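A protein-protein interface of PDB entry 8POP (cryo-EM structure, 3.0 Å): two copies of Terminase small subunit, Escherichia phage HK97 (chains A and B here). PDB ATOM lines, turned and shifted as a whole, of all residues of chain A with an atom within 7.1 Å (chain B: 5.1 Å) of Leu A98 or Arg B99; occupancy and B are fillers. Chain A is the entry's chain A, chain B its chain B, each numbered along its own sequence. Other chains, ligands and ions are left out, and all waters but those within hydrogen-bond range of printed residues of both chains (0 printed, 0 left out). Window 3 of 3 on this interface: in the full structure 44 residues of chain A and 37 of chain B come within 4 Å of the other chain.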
ATOM      1  N   TYR A  71     -15.351  -0.986   7.768  1.00  0.00           N
ATOM      2  CA  TYR A  71     -16.511  -1.729   8.219  1.00  0.00           C
ATOM      3  C   TYR A  71     -17.769  -1.339   7.442  1.00  0.00           C
ATOM      4  O   TYR A  71     -18.697  -2.139   7.362  1.00  0.00           O
ATOM      5  CB  TYR A  71     -16.719  -1.539   9.725  1.00  0.00           C
ATOM      6  CG  TYR A  71     -17.642  -2.552  10.363  1.00  0.00           C
ATOM      7  CD1 TYR A  71     -17.498  -3.915  10.120  1.00  0.00           C
ATOM      8  CD2 TYR A  71     -18.650  -2.163  11.227  1.00  0.00           C
ATOM      9  CE1 TYR A  71     -18.353  -4.845  10.674  1.00  0.00           C
ATOM     10  CE2 TYR A  71     -19.473  -3.095  11.839  1.00  0.00           C
ATOM     11  CZ  TYR A  71     -19.338  -4.437  11.549  1.00  0.00           C
ATOM     12  OH  TYR A  71     -20.184  -5.351  12.137  1.00  0.00           O
ATOM     13  N   VAL A  74     -18.192  -3.659   4.543  1.00  0.00           N
ATOM     14  CA  VAL A  74     -18.636  -4.974   4.970  1.00  0.00           C
ATOM     15  C   VAL A  74     -20.143  -5.006   5.190  1.00  0.00           C
ATOM     16  O   VAL A  74     -20.789  -5.955   4.762  1.00  0.00           O
ATOM     17  CB  VAL A  74     -17.903  -5.387   6.252  1.00  0.00           C
ATOM     18  CG1 VAL A  74     -18.443  -6.687   6.818  1.00  0.00           C
ATOM     19  CG2 VAL A  74     -16.400  -5.459   6.022  1.00  0.00           C
ATOM     20  N   LEU A  75     -20.695  -4.006   5.901  1.00  0.00           N
ATOM     21  CA  LEU A  75     -22.125  -3.970   6.173  1.00  0.00           C
ATOM     22  C   LEU A  75     -22.892  -3.783   4.874  1.00  0.00           C
ATOM     23  O   LEU A  75     -23.956  -4.359   4.707  1.00  0.00           O
ATOM     24  CB  LEU A  75     -22.464  -2.824   7.112  1.00  0.00           C
ATOM     25  CG  LEU A  75     -21.972  -2.933   8.537  1.00  0.00           C
ATOM     26  CD1 LEU A  75     -22.393  -1.717   9.339  1.00  0.00           C
ATOM     27  CD2 LEU A  75     -22.512  -4.168   9.149  1.00  0.00           C
ATOM     28  N   ARG A  76     -22.364  -2.980   3.956  1.00  0.00           N
ATOM     29  CA  ARG A  76     -23.107  -2.726   2.739  1.00  0.00           C
ATOM     30  C   ARG A  76     -23.249  -4.031   1.949  1.00  0.00           C
ATOM     31  O   ARG A  76     -24.309  -4.281   1.376  1.00  0.00           O
ATOM     32  CB  ARG A  76     -22.476  -1.597   1.935  1.00  0.00           C
ATOM     33  CG  ARG A  76     -23.241  -1.240   0.675  1.00  0.00           C
ATOM     34  CD  ARG A  76     -22.524  -0.144  -0.097  1.00  0.00           C
ATOM     35  NE  ARG A  76     -22.675   1.145   0.551  1.00  0.00           N
ATOM     36  CZ  ARG A  76     -21.683   1.986   0.831  1.00  0.00           C
ATOM     37  NH1 ARG A  76     -20.413   1.631   0.682  1.00  0.00           N
ATOM     38  NH2 ARG A  76     -21.966   3.202   1.280  1.00  0.00           N
ATOM     39  N   LYS A  77     -22.212  -4.872   1.953  1.00  0.00           N
ATOM     40  CA  LYS A  77     -22.298  -6.168   1.299  1.00  0.00           C
ATOM     41  C   LYS A  77     -23.399  -7.014   1.935  1.00  0.00           C
ATOM     42  O   LYS A  77     -24.191  -7.636   1.223  1.00  0.00           O
ATOM     43  CB  LYS A  77     -20.974  -6.930   1.354  1.00  0.00           C
ATOM     44  CG  LYS A  77     -19.945  -6.434   0.350  1.00  0.00           C
ATOM     45  CD  LYS A  77     -18.669  -7.226   0.325  1.00  0.00           C
ATOM     46  CE  LYS A  77     -17.836  -6.919  -0.906  1.00  0.00           C
ATOM     47  NZ  LYS A  77     -16.582  -7.711  -0.940  1.00  0.00           N
ATOM     48  N   ASP A  78     -23.441  -7.032   3.270  1.00  0.00           N
ATOM     49  CA  ASP A  78     -24.460  -7.778   3.992  1.00  0.00           C
ATOM     50  C   ASP A  78     -25.856  -7.318   3.574  1.00  0.00           C
ATOM     51  O   ASP A  78     -26.752  -8.140   3.419  1.00  0.00           O
ATOM     52  CB  ASP A  78     -24.301  -7.622   5.506  1.00  0.00           C
ATOM     53  CG  ASP A  78     -25.251  -8.449   6.354  1.00  0.00           C
ATOM     54  OD1 ASP A  78     -26.143  -9.105   5.775  1.00  0.00           O
ATOM     55  OD2 ASP A  78     -25.070  -8.453   7.589  1.00  0.00           O
ATOM     56  N   LEU A  79     -26.039  -6.006   3.414  1.00  0.00           N
ATOM     57  CA  LEU A  79     -27.347  -5.456   3.141  1.00  0.00           C
ATOM     58  C   LEU A  79     -27.813  -5.869   1.758  1.00  0.00           C
ATOM     59  O   LEU A  79     -28.988  -6.195   1.595  1.00  0.00           O
ATOM     60  CB  LEU A  79     -27.286  -3.931   3.235  1.00  0.00           C
ATOM     61  CG  LEU A  79     -28.568  -3.191   2.844  1.00  0.00           C
ATOM     62  CD1 LEU A  79     -29.717  -3.552   3.767  1.00  0.00           C
ATOM     63  CD2 LEU A  79     -28.355  -1.693   2.880  1.00  0.00           C
ATOM     64  N   ARG A  80     -26.913  -5.821   0.762  1.00  0.00           N
ATOM     65  CA  ARG A  80     -27.285  -6.126  -0.614  1.00  0.00           C
ATOM     66  C   ARG A  80     -27.747  -7.578  -0.738  1.00  0.00           C
ATOM     67  O   ARG A  80     -28.651  -7.868  -1.526  1.00  0.00           O
ATOM     68  CB  ARG A  80     -26.132  -5.835  -1.575  1.00  0.00           C
ATOM     69  CG  ARG A  80     -25.791  -4.355  -1.714  1.00  0.00           C
ATOM     70  CD  ARG A  80     -26.790  -3.574  -2.550  1.00  0.00           C
ATOM     71  NE  ARG A  80     -26.564  -2.134  -2.502  1.00  0.00           N
ATOM     72  CZ  ARG A  80     -26.985  -1.311  -1.541  1.00  0.00           C
ATOM     73  NH1 ARG A  80     -27.761  -1.755  -0.570  1.00  0.00           N
ATOM     74  NH2 ARG A  80     -26.658  -0.028  -1.567  1.00  0.00           N
ATOM     75  N   GLU A  82     -29.351  -9.330   1.677  1.00  0.00           N
ATOM     76  CA  GLU A  82     -30.674  -9.465   2.267  1.00  0.00           C
ATOM     77  C   GLU A  82     -31.740  -8.848   1.368  1.00  0.00           C
ATOM     78  O   GLU A  82     -32.894  -9.265   1.415  1.00  0.00           O
ATOM     79  CB  GLU A  82     -30.755  -8.774   3.629  1.00  0.00           C
ATOM     80  CG  GLU A  82     -29.794  -9.317   4.664  1.00  0.00           C
ATOM     81  CD  GLU A  82     -29.928 -10.803   4.931  1.00  0.00           C
ATOM     82  OE1 GLU A  82     -31.079 -11.261   5.132  1.00  0.00           O
ATOM     83  OE2 GLU A  82     -28.881 -11.500   4.960  1.00  0.00           O
ATOM     84  N   GLY A  93     -36.963  -6.777   9.200  1.00  0.00           N
ATOM     85  CA  GLY A  93     -36.392  -6.266  10.438  1.00  0.00           C
ATOM     86  C   GLY A  93     -34.875  -6.104  10.358  1.00  0.00           C
ATOM     87  O   GLY A  93     -34.327  -5.108  10.830  1.00  0.00           O
ATOM     88  N   LEU A  94     -34.209  -7.092   9.757  1.00  0.00           N
ATOM     89  CA  LEU A  94     -32.771  -7.050   9.587  1.00  0.00           C
ATOM     90  C   LEU A  94     -32.414  -5.999   8.552  1.00  0.00           C
ATOM     91  O   LEU A  94     -31.399  -5.321   8.682  1.00  0.00           O
ATOM     92  CB  LEU A  94     -32.264  -8.424   9.142  1.00  0.00           C
ATOM     93  CG  LEU A  94     -30.766  -8.499   8.843  1.00  0.00           C
ATOM     94  CD1 LEU A  94     -29.932  -8.207  10.083  1.00  0.00           C
ATOM     95  CD2 LEU A  94     -30.376  -9.858   8.311  1.00  0.00           C
ATOM     96  N   ILE A  95     -33.233  -5.886   7.509  1.00  0.00           N
ATOM     97  CA  ILE A  95     -32.967  -4.900   6.483  1.00  0.00           C
ATOM     98  C   ILE A  95     -32.999  -3.520   7.110  1.00  0.00           C
ATOM     99  O   ILE A  95     -32.117  -2.702   6.829  1.00  0.00           O
ATOM    100  CB  ILE A  95     -33.935  -5.047   5.296  1.00  0.00           C
ATOM    101  CG1 ILE A  95     -33.583  -6.292   4.474  1.00  0.00           C
ATOM    102  CG2 ILE A  95     -33.963  -3.790   4.432  1.00  0.00           C
ATOM    103  CD1 ILE A  95     -34.583  -6.603   3.389  1.00  0.00           C
ATOM    104  N   LYS A  96     -33.990  -3.280   7.977  1.00  0.00           N
ATOM    105  CA  LYS A  96     -34.141  -1.976   8.611  1.00  0.00           C
ATOM    106  C   LYS A  96     -32.916  -1.672   9.476  1.00  0.00           C
ATOM    107  O   LYS A  96     -32.430  -0.545   9.472  1.00  0.00           O
ATOM    108  CB  LYS A  96     -35.447  -1.933   9.405  1.00  0.00           C
ATOM    109  CG  LYS A  96     -35.737  -0.607  10.092  1.00  0.00           C
ATOM    110  CD  LYS A  96     -37.175  -0.432  10.529  1.00  0.00           C
ATOM    111  CE  LYS A  96     -37.623  -1.366  11.636  1.00  0.00           C
ATOM    112  NZ  LYS A  96     -39.101  -1.522  11.658  1.00  0.00           N
ATOM    113  N   ASP A  97     -32.402  -2.687  10.180  1.00  0.00           N
ATOM    114  CA  ASP A  97     -31.291  -2.492  11.093  1.00  0.00           C
ATOM    115  C   ASP A  97     -30.007  -2.192  10.329  1.00  0.00           C
ATOM    116  O   ASP A  97     -29.271  -1.286  10.714  1.00  0.00           O
ATOM    117  CB  ASP A  97     -31.100  -3.704  12.000  1.00  0.00           C
ATOM    118  CG  ASP A  97     -32.242  -3.906  12.984  1.00  0.00           C
ATOM    119  OD1 ASP A  97     -33.076  -2.973  13.122  1.00  0.00           O
ATOM    120  OD2 ASP A  97     -32.302  -5.001  13.596  1.00  0.00           O
ATOM    121  N   LEU A  98     -29.739  -2.950   9.263  1.00  0.00           N
ATOM    122  CA  LEU A  98     -28.530  -2.725   8.491  1.00  0.00           C
ATOM    123  C   LEU A  98     -28.520  -1.319   7.898  1.00  0.00           C
ATOM    124  O   LEU A  98     -27.464  -0.671   7.857  1.00  0.00           O
ATOM    125  CB  LEU A  98     -28.417  -3.768   7.385  1.00  0.00           C
ATOM    126  CG  LEU A  98     -27.874  -5.119   7.848  1.00  0.00           C
ATOM    127  CD1 LEU A  98     -27.980  -6.150   6.757  1.00  0.00           C
ATOM    128  CD2 LEU A  98     -26.434  -5.023   8.284  1.00  0.00           C
ATOM    129  N   ARG A  99     -29.696  -0.844   7.462  1.00  0.00           N
ATOM    130  CA  ARG A  99     -29.780   0.479   6.880  1.00  0.00           C
ATOM    131  C   ARG A  99     -29.409   1.523   7.927  1.00  0.00           C
ATOM    132  O   ARG A  99     -28.667   2.464   7.606  1.00  0.00           O
ATOM    133  CB  ARG A  99     -31.168   0.726   6.291  1.00  0.00           C
ATOM    134  CG  ARG A  99     -31.363   0.107   4.916  1.00  0.00           C
ATOM    135  CD  ARG A  99     -32.797   0.206   4.440  1.00  0.00           C
ATOM    136  NE  ARG A  99     -32.969  -0.452   3.147  1.00  0.00           N
ATOM    137  CZ  ARG A  99     -34.141  -0.764   2.611  1.00  0.00           C
ATOM    138  NH1 ARG A  99     -35.257  -0.508   3.270  1.00  0.00           N
ATOM    139  NH2 ARG A  99     -34.202  -1.335   1.424  1.00  0.00           N
ATOM    140  N   LYS A 100     -29.898   1.355   9.175  1.00  0.00           N
ATOM    141  CA  LYS A 100     -29.621   2.336  10.213  1.00  0.00           C
ATOM    142  C   LYS A 100     -28.158   2.292  10.635  1.00  0.00           C
ATOM    143  O   LYS A 100     -27.546   3.343  10.815  1.00  0.00           O
ATOM    144  CB  LYS A 100     -30.495   2.113  11.439  1.00  0.00           C
ATOM    145  CG  LYS A 100     -31.904   2.677  11.344  1.00  0.00           C
ATOM    146  CD  LYS A 100     -32.791   2.090  12.432  1.00  0.00           C
ATOM    147  CE  LYS A 100     -34.287   2.236  12.220  1.00  0.00           C
ATOM    148  NZ  LYS A 100     -35.052   1.532  13.279  1.00  0.00           N
ATOM    149  N   GLN A 101     -27.587   1.090  10.779  1.00  0.00           N
ATOM    150  CA  GLN A 101     -26.204   0.977  11.208  1.00  0.00           C
ATOM    151  C   GLN A 101     -25.286   1.691  10.223  1.00  0.00           C
ATOM    152  O   GLN A 101     -24.259   2.221  10.635  1.00  0.00           O
ATOM    153  CB  GLN A 101     -25.791  -0.486  11.372  1.00  0.00           C
ATOM    154  CG  GLN A 101     -26.430  -1.135  12.590  1.00  0.00           C
ATOM    155  CD  GLN A 101     -26.326  -2.643  12.612  1.00  0.00           C
ATOM    156  OE1 GLN A 101     -25.713  -3.265  11.747  1.00  0.00           O
ATOM    157  NE2 GLN A 101     -26.956  -3.248  13.607  1.00  0.00           N
ATOM    158  N   ILE A 102     -25.649   1.702   8.935  1.00  0.00           N
ATOM    159  CA  ILE A 102     -24.771   2.292   7.949  1.00  0.00           C
ATOM    160  C   ILE A 102     -24.791   3.814   8.084  1.00  0.00           C
ATOM    161  O   ILE A 102     -23.756   4.459   7.938  1.00  0.00           O
ATOM    162  CB  ILE A 102     -25.113   1.808   6.530  1.00  0.00           C
ATOM    163  CG1 ILE A 102     -24.744   0.334   6.359  1.00  0.00           C
ATOM    164  CG2 ILE A 102     -24.427   2.676   5.477  1.00  0.00           C
ATOM    165  CD1 ILE A 102     -25.090  -0.243   4.987  1.00  0.00           C
ATOM    166  N   VAL A 103     -25.950   4.399   8.384  1.00  0.00           N
ATOM    167  CA  VAL A 103     -26.012   5.845   8.547  1.00  0.00           C
ATOM    168  C   VAL A 103     -25.277   6.289   9.817  1.00  0.00           C
ATOM    169  O   VAL A 103     -24.564   7.295   9.791  1.00  0.00           O
ATOM    170  CB  VAL A 103     -27.465   6.343   8.515  1.00  0.00           C
ATOM    171  CG1 VAL A 103     -27.601   7.725   9.124  1.00  0.00           C
ATOM    172  CG2 VAL A 103     -27.998   6.354   7.101  1.00  0.00           C
ATOM    173  N   GLU A 104     -25.429   5.541  10.918  1.00  0.00           N
ATOM    174  CA  GLU A 104     -24.733   5.868  12.153  1.00  0.00           C
ATOM    175  C   GLU A 104     -23.224   5.885  11.923  1.00  0.00           C
ATOM    176  O   GLU A 104     -22.554   6.807  12.383  1.00  0.00           O
ATOM    177  CB  GLU A 104     -25.065   4.858  13.248  1.00  0.00           C
ATOM    178  CG  GLU A 104     -24.445   5.142  14.600  1.00  0.00           C
ATOM    179  CD  GLU A 104     -24.718   6.532  15.138  1.00  0.00           C
ATOM    180  OE1 GLU A 104     -25.849   7.039  14.934  1.00  0.00           O
ATOM    181  OE2 GLU A 104     -23.808   7.106  15.783  1.00  0.00           O
ATOM    182  N   LEU A 105     -22.675   4.869  11.246  1.00  0.00           N
ATOM    183  CA  LEU A 105     -21.246   4.864  10.982  1.00  0.00           C
ATOM    184  C   LEU A 105     -20.855   6.106  10.185  1.00  0.00           C
ATOM    185  O   LEU A 105     -19.859   6.749  10.496  1.00  0.00           O
ATOM    186  CB  LEU A 105     -20.835   3.604  10.216  1.00  0.00           C
ATOM    187  CG  LEU A 105     -20.457   2.400  11.075  1.00  0.00           C
ATOM    188  CD1 LEU A 105     -19.976   1.229  10.214  1.00  0.00           C
ATOM    189  CD2 LEU A 105     -19.387   2.739  12.082  1.00  0.00           C
ATOM    190  N   LEU B  79     -17.324  -9.183  18.697  1.00  0.00           N
ATOM    191  CA  LEU B  79     -18.251  -9.030  17.597  1.00  0.00           C
ATOM    192  C   LEU B  79     -17.870  -9.939  16.446  1.00  0.00           C
ATOM    193  O   LEU B  79     -18.753 -10.536  15.840  1.00  0.00           O
ATOM    194  CB  LEU B  79     -18.256  -7.573  17.143  1.00  0.00           C
ATOM    195  CG  LEU B  79     -19.099  -7.269  15.914  1.00  0.00           C
ATOM    196  CD1 LEU B  79     -20.566  -7.546  16.200  1.00  0.00           C
ATOM    197  CD2 LEU B  79     -18.870  -5.820  15.490  1.00  0.00           C
ATOM    198  N   GLU B  83     -20.141 -12.888  14.437  1.00  0.00           N
ATOM    199  CA  GLU B  83     -20.481 -12.708  13.041  1.00  0.00           C
ATOM    200  C   GLU B  83     -20.103 -13.948  12.227  1.00  0.00           C
ATOM    201  O   GLU B  83     -20.568 -14.110  11.109  1.00  0.00           O
ATOM    202  CB  GLU B  83     -19.777 -11.474  12.486  1.00  0.00           C
ATOM    203  CG  GLU B  83     -20.417 -10.152  12.879  1.00  0.00           C
ATOM    204  CD  GLU B  83     -19.754  -8.929  12.249  1.00  0.00           C
ATOM    205  OE1 GLU B  83     -20.384  -7.850  12.245  1.00  0.00           O
ATOM    206  OE2 GLU B  83     -18.593  -9.037  11.784  1.00  0.00           O
ATOM    207  N   LEU B  94     -27.628  -9.817  19.691  1.00  0.00           N
ATOM    208  CA  LEU B  94     -26.351  -9.524  20.306  1.00  0.00           C
ATOM    209  C   LEU B  94     -25.461  -8.795  19.307  1.00  0.00           C
ATOM    210  O   LEU B  94     -24.709  -7.902  19.689  1.00  0.00           O
ATOM    211  CB  LEU B  94     -25.684 -10.822  20.751  1.00  0.00           C
ATOM    212  CG  LEU B  94     -24.277 -10.675  21.330  1.00  0.00           C
ATOM    213  CD1 LEU B  94     -24.291  -9.836  22.605  1.00  0.00           C
ATOM    214  CD2 LEU B  94     -23.662 -12.046  21.592  1.00  0.00           C
ATOM    215  N   ILE B  95     -25.535  -9.197  18.039  1.00  0.00           N
ATOM    216  CA  ILE B  95     -24.721  -8.557  17.029  1.00  0.00           C
ATOM    217  C   ILE B  95     -25.104  -7.077  16.961  1.00  0.00           C
ATOM    218  O   ILE B  95     -24.217  -6.203  16.907  1.00  0.00           O
ATOM    219  CB  ILE B  95     -24.839  -9.269  15.674  1.00  0.00           C
ATOM    220  CG1 ILE B  95     -24.117 -10.615  15.716  1.00  0.00           C
ATOM    221  CG2 ILE B  95     -24.301  -8.393  14.551  1.00  0.00           C
ATOM    222  CD1 ILE B  95     -24.314 -11.460  14.464  1.00  0.00           C
ATOM    223  N   LYS B  96     -26.416  -6.802  16.994  1.00  0.00           N
ATOM    224  CA  LYS B  96     -26.896  -5.436  16.900  1.00  0.00           C
ATOM    225  C   LYS B  96     -26.392  -4.609  18.089  1.00  0.00           C
ATOM    226  O   LYS B  96     -25.988  -3.451  17.918  1.00  0.00           O
ATOM    227  CB  LYS B  96     -28.422  -5.430  16.800  1.00  0.00           C
ATOM    228  CG  LYS B  96     -29.069  -4.061  16.665  1.00  0.00           C
ATOM    229  CD  LYS B  96     -30.552  -4.152  16.390  1.00  0.00           C
ATOM    230  CE  LYS B  96     -31.172  -2.777  16.255  1.00  0.00           C
ATOM    231  NZ  LYS B  96     -32.655  -2.818  16.228  1.00  0.00           N
ATOM    232  N   ASP B  97     -26.382  -5.218  19.285  1.00  0.00           N
ATOM    233  CA  ASP B  97     -26.009  -4.505  20.490  1.00  0.00           C
ATOM    234  C   ASP B  97     -24.519  -4.188  20.482  1.00  0.00           C
ATOM    235  O   ASP B  97     -24.125  -3.082  20.847  1.00  0.00           O
ATOM    236  CB  ASP B  97     -26.378  -5.301  21.737  1.00  0.00           C
ATOM    237  CG  ASP B  97     -25.952  -4.630  23.034  1.00  0.00           C
ATOM    238  OD1 ASP B  97     -25.579  -3.429  22.988  1.00  0.00           O
ATOM    239  OD2 ASP B  97     -25.974  -5.322  24.081  1.00  0.00           O
ATOM    240  N   LEU B  98     -23.689  -5.161  20.107  1.00  0.00           N
ATOM    241  CA  LEU B  98     -22.254  -4.935  20.101  1.00  0.00           C
ATOM    242  C   LEU B  98     -21.913  -3.813  19.125  1.00  0.00           C
ATOM    243  O   LEU B  98     -21.019  -3.025  19.392  1.00  0.00           O
ATOM    244  CB  LEU B  98     -21.525  -6.226  19.719  1.00  0.00           C
ATOM    245  CG  LEU B  98     -21.374  -7.239  20.847  1.00  0.00           C
ATOM    246  CD1 LEU B  98     -20.782  -8.535  20.289  1.00  0.00           C
ATOM    247  CD2 LEU B  98     -20.524  -6.718  21.988  1.00  0.00           C
ATOM    248  N   ARG B  99     -22.607  -3.759  17.987  1.00  0.00           N
ATOM    249  CA  ARG B  99     -22.329  -2.724  17.011  1.00  0.00           C
ATOM    250  C   ARG B  99     -22.640  -1.346  17.604  1.00  0.00           C
ATOM    251  O   ARG B  99     -21.861  -0.409  17.409  1.00  0.00           O
ATOM    252  CB  ARG B  99     -23.084  -2.987  15.708  1.00  0.00           C
ATOM    253  CG  ARG B  99     -22.430  -4.040  14.821  1.00  0.00           C
ATOM    254  CD  ARG B  99     -23.300  -4.388  13.642  1.00  0.00           C
ATOM    255  NE  ARG B  99     -22.791  -5.471  12.824  1.00  0.00           N
ATOM    256  CZ  ARG B  99     -23.521  -6.144  11.932  1.00  0.00           C
ATOM    257  NH1 ARG B  99     -24.821  -5.923  11.827  1.00  0.00           N
ATOM    258  NH2 ARG B  99     -22.969  -7.051  11.141  1.00  0.00           N
ATOM    259  N   LYS B 100     -23.745  -1.220  18.350  1.00  0.00           N
ATOM    260  CA  LYS B 100     -24.101   0.059  18.952  1.00  0.00           C
ATOM    261  C   LYS B 100     -23.124   0.454  20.071  1.00  0.00           C
ATOM    262  O   LYS B 100     -22.696   1.607  20.155  1.00  0.00           O
ATOM    263  CB  LYS B 100     -25.521   0.022  19.507  1.00  0.00           C
ATOM    264  CG  LYS B 100     -26.236   1.352  19.633  1.00  0.00           C
ATOM    265  CD  LYS B 100     -26.697   1.913  18.296  1.00  0.00           C
ATOM    266  CE  LYS B 100     -27.619   3.107  18.430  1.00  0.00           C
ATOM    267  NZ  LYS B 100     -27.814   3.805  17.131  1.00  0.00           N
ATOM    268  N   GLN B 101     -22.752  -0.503  20.917  1.00  0.00           N
ATOM    269  CA  GLN B 101     -21.850  -0.204  22.013  1.00  0.00           C
ATOM    270  C   GLN B 101     -20.518   0.310  21.475  1.00  0.00           C
ATOM    271  O   GLN B 101     -19.854   1.086  22.141  1.00  0.00           O
ATOM    272  CB  GLN B 101     -21.629  -1.436  22.899  1.00  0.00           C
ATOM    273  CG  GLN B 101     -22.848  -1.781  23.731  1.00  0.00           C
ATOM    274  CD  GLN B 101     -22.773  -3.140  24.382  1.00  0.00           C
ATOM    275  OE1 GLN B 101     -21.745  -3.810  24.358  1.00  0.00           O
ATOM    276  NE2 GLN B 101     -23.853  -3.540  25.033  1.00  0.00           N
ATOM    277  N   ILE B 102     -20.104  -0.145  20.291  1.00  0.00           N
ATOM    278  CA  ILE B 102     -18.815   0.257  19.764  1.00  0.00           C
ATOM    279  C   ILE B 102     -18.869   1.717  19.319  1.00  0.00           C
ATOM    280  O   ILE B 102     -17.900   2.459  19.511  1.00  0.00           O
ATOM    281  CB  ILE B 102     -18.333  -0.706  18.668  1.00  0.00           C
ATOM    282  CG1 ILE B 102     -17.908  -2.041  19.305  1.00  0.00           C
ATOM    283  CG2 ILE B 102     -17.212  -0.099  17.846  1.00  0.00           C
ATOM    284  CD1 ILE B 102     -17.440  -3.113  18.312  1.00  0.00           C
ATOM    285  N   VAL B 103     -19.996   2.150  18.751  1.00  0.00           N
ATOM    286  CA  VAL B 103     -20.100   3.539  18.340  1.00  0.00           C
ATOM    287  C   VAL B 103     -20.174   4.468  19.558  1.00  0.00           C
ATOM    288  O   VAL B 103     -19.546   5.533  19.566  1.00  0.00           O
ATOM    289  CB  VAL B 103     -21.270   3.729  17.372  1.00  0.00           C
ATOM    290  CG1 VAL B 103     -21.705   5.179  17.283  1.00  0.00           C
ATOM    291  CG2 VAL B 103     -20.888   3.195  15.995  1.00  0.00           C
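OH of Tyr A71 lies within hydrogen-bond range of OE1 of Glu B83, 2.5 Å away. The side-chain amide oxygen (OE1) of Gln A101 is in hydrogen-bond range of the guanidinium group (NH1) of Arg B99. OD1 of Asp A97 is in salt-bridge range of NZ of Lys B96, at 3.1 Å. OH of Tyr A71 sits at hydrogen-bond distance from NE of Arg B99.
The guanidinium group of Arg B99 is in salt-bridge range of the side-chain carboxylate of Glu B83.
Tyr A71 touches Leu B79. Arg B99 touches Leu A75. Arg B99 touches Leu A98. Gln A101 touches Lys B96. Val B103 touches Glu A104.
Of the printed residues of chain B, Asp A97 touches Lys B96 (3.1 Å). Val A103 touches none of the printed residues of chain B. Printed residues of chain B within 4 Å of Glu A104: Val B103. Printed residues of chain A within 4 Å of Leu B79: Tyr A71. Of the printed residues of chain A, Arg B99 touches Tyr A71, Leu A75, Leu A98 and Gln A101. The nearest printed residue of chain B that does not touch Leu A98 is Lys B96 (7.1 Å). The nearest printed residue of chain A that does not touch Arg B99 is Asp A78 (4.4 Å). The nearest printed residue of chain A that does not touch Lys B96 is Lys A100 (5.8 Å).
Hydrophobic or aromatic side chains of chain A that line the printed part of chain B: Tyr A71, Leu A75 and Leu A98. Among the printed residues, 9 pairs touch across the chains. Among the printed residues, Asp or Glu carboxylates within 4 Å of a Lys or Arg side-chain nitrogen of the other chain: Asp A97 with Lys B96.
Asp A97 touches Lys B96, but with the chains exchanged Lys A96 does not touch Asp B97 (12.3 Å). Leu A98 touches Arg B99, but with the chains exchanged Arg A99 does not touch Leu B98 (14.3 Å). Gln A101 touches Lys B96, but with the chains exchanged Lys A96 does not touch Gln B101 (15.0 Å). Gln A101 touches Arg B99, but with the chains exchanged Arg A99 does not touch Gln B101 (14.7 Å). 11 positions are printed for both chains.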
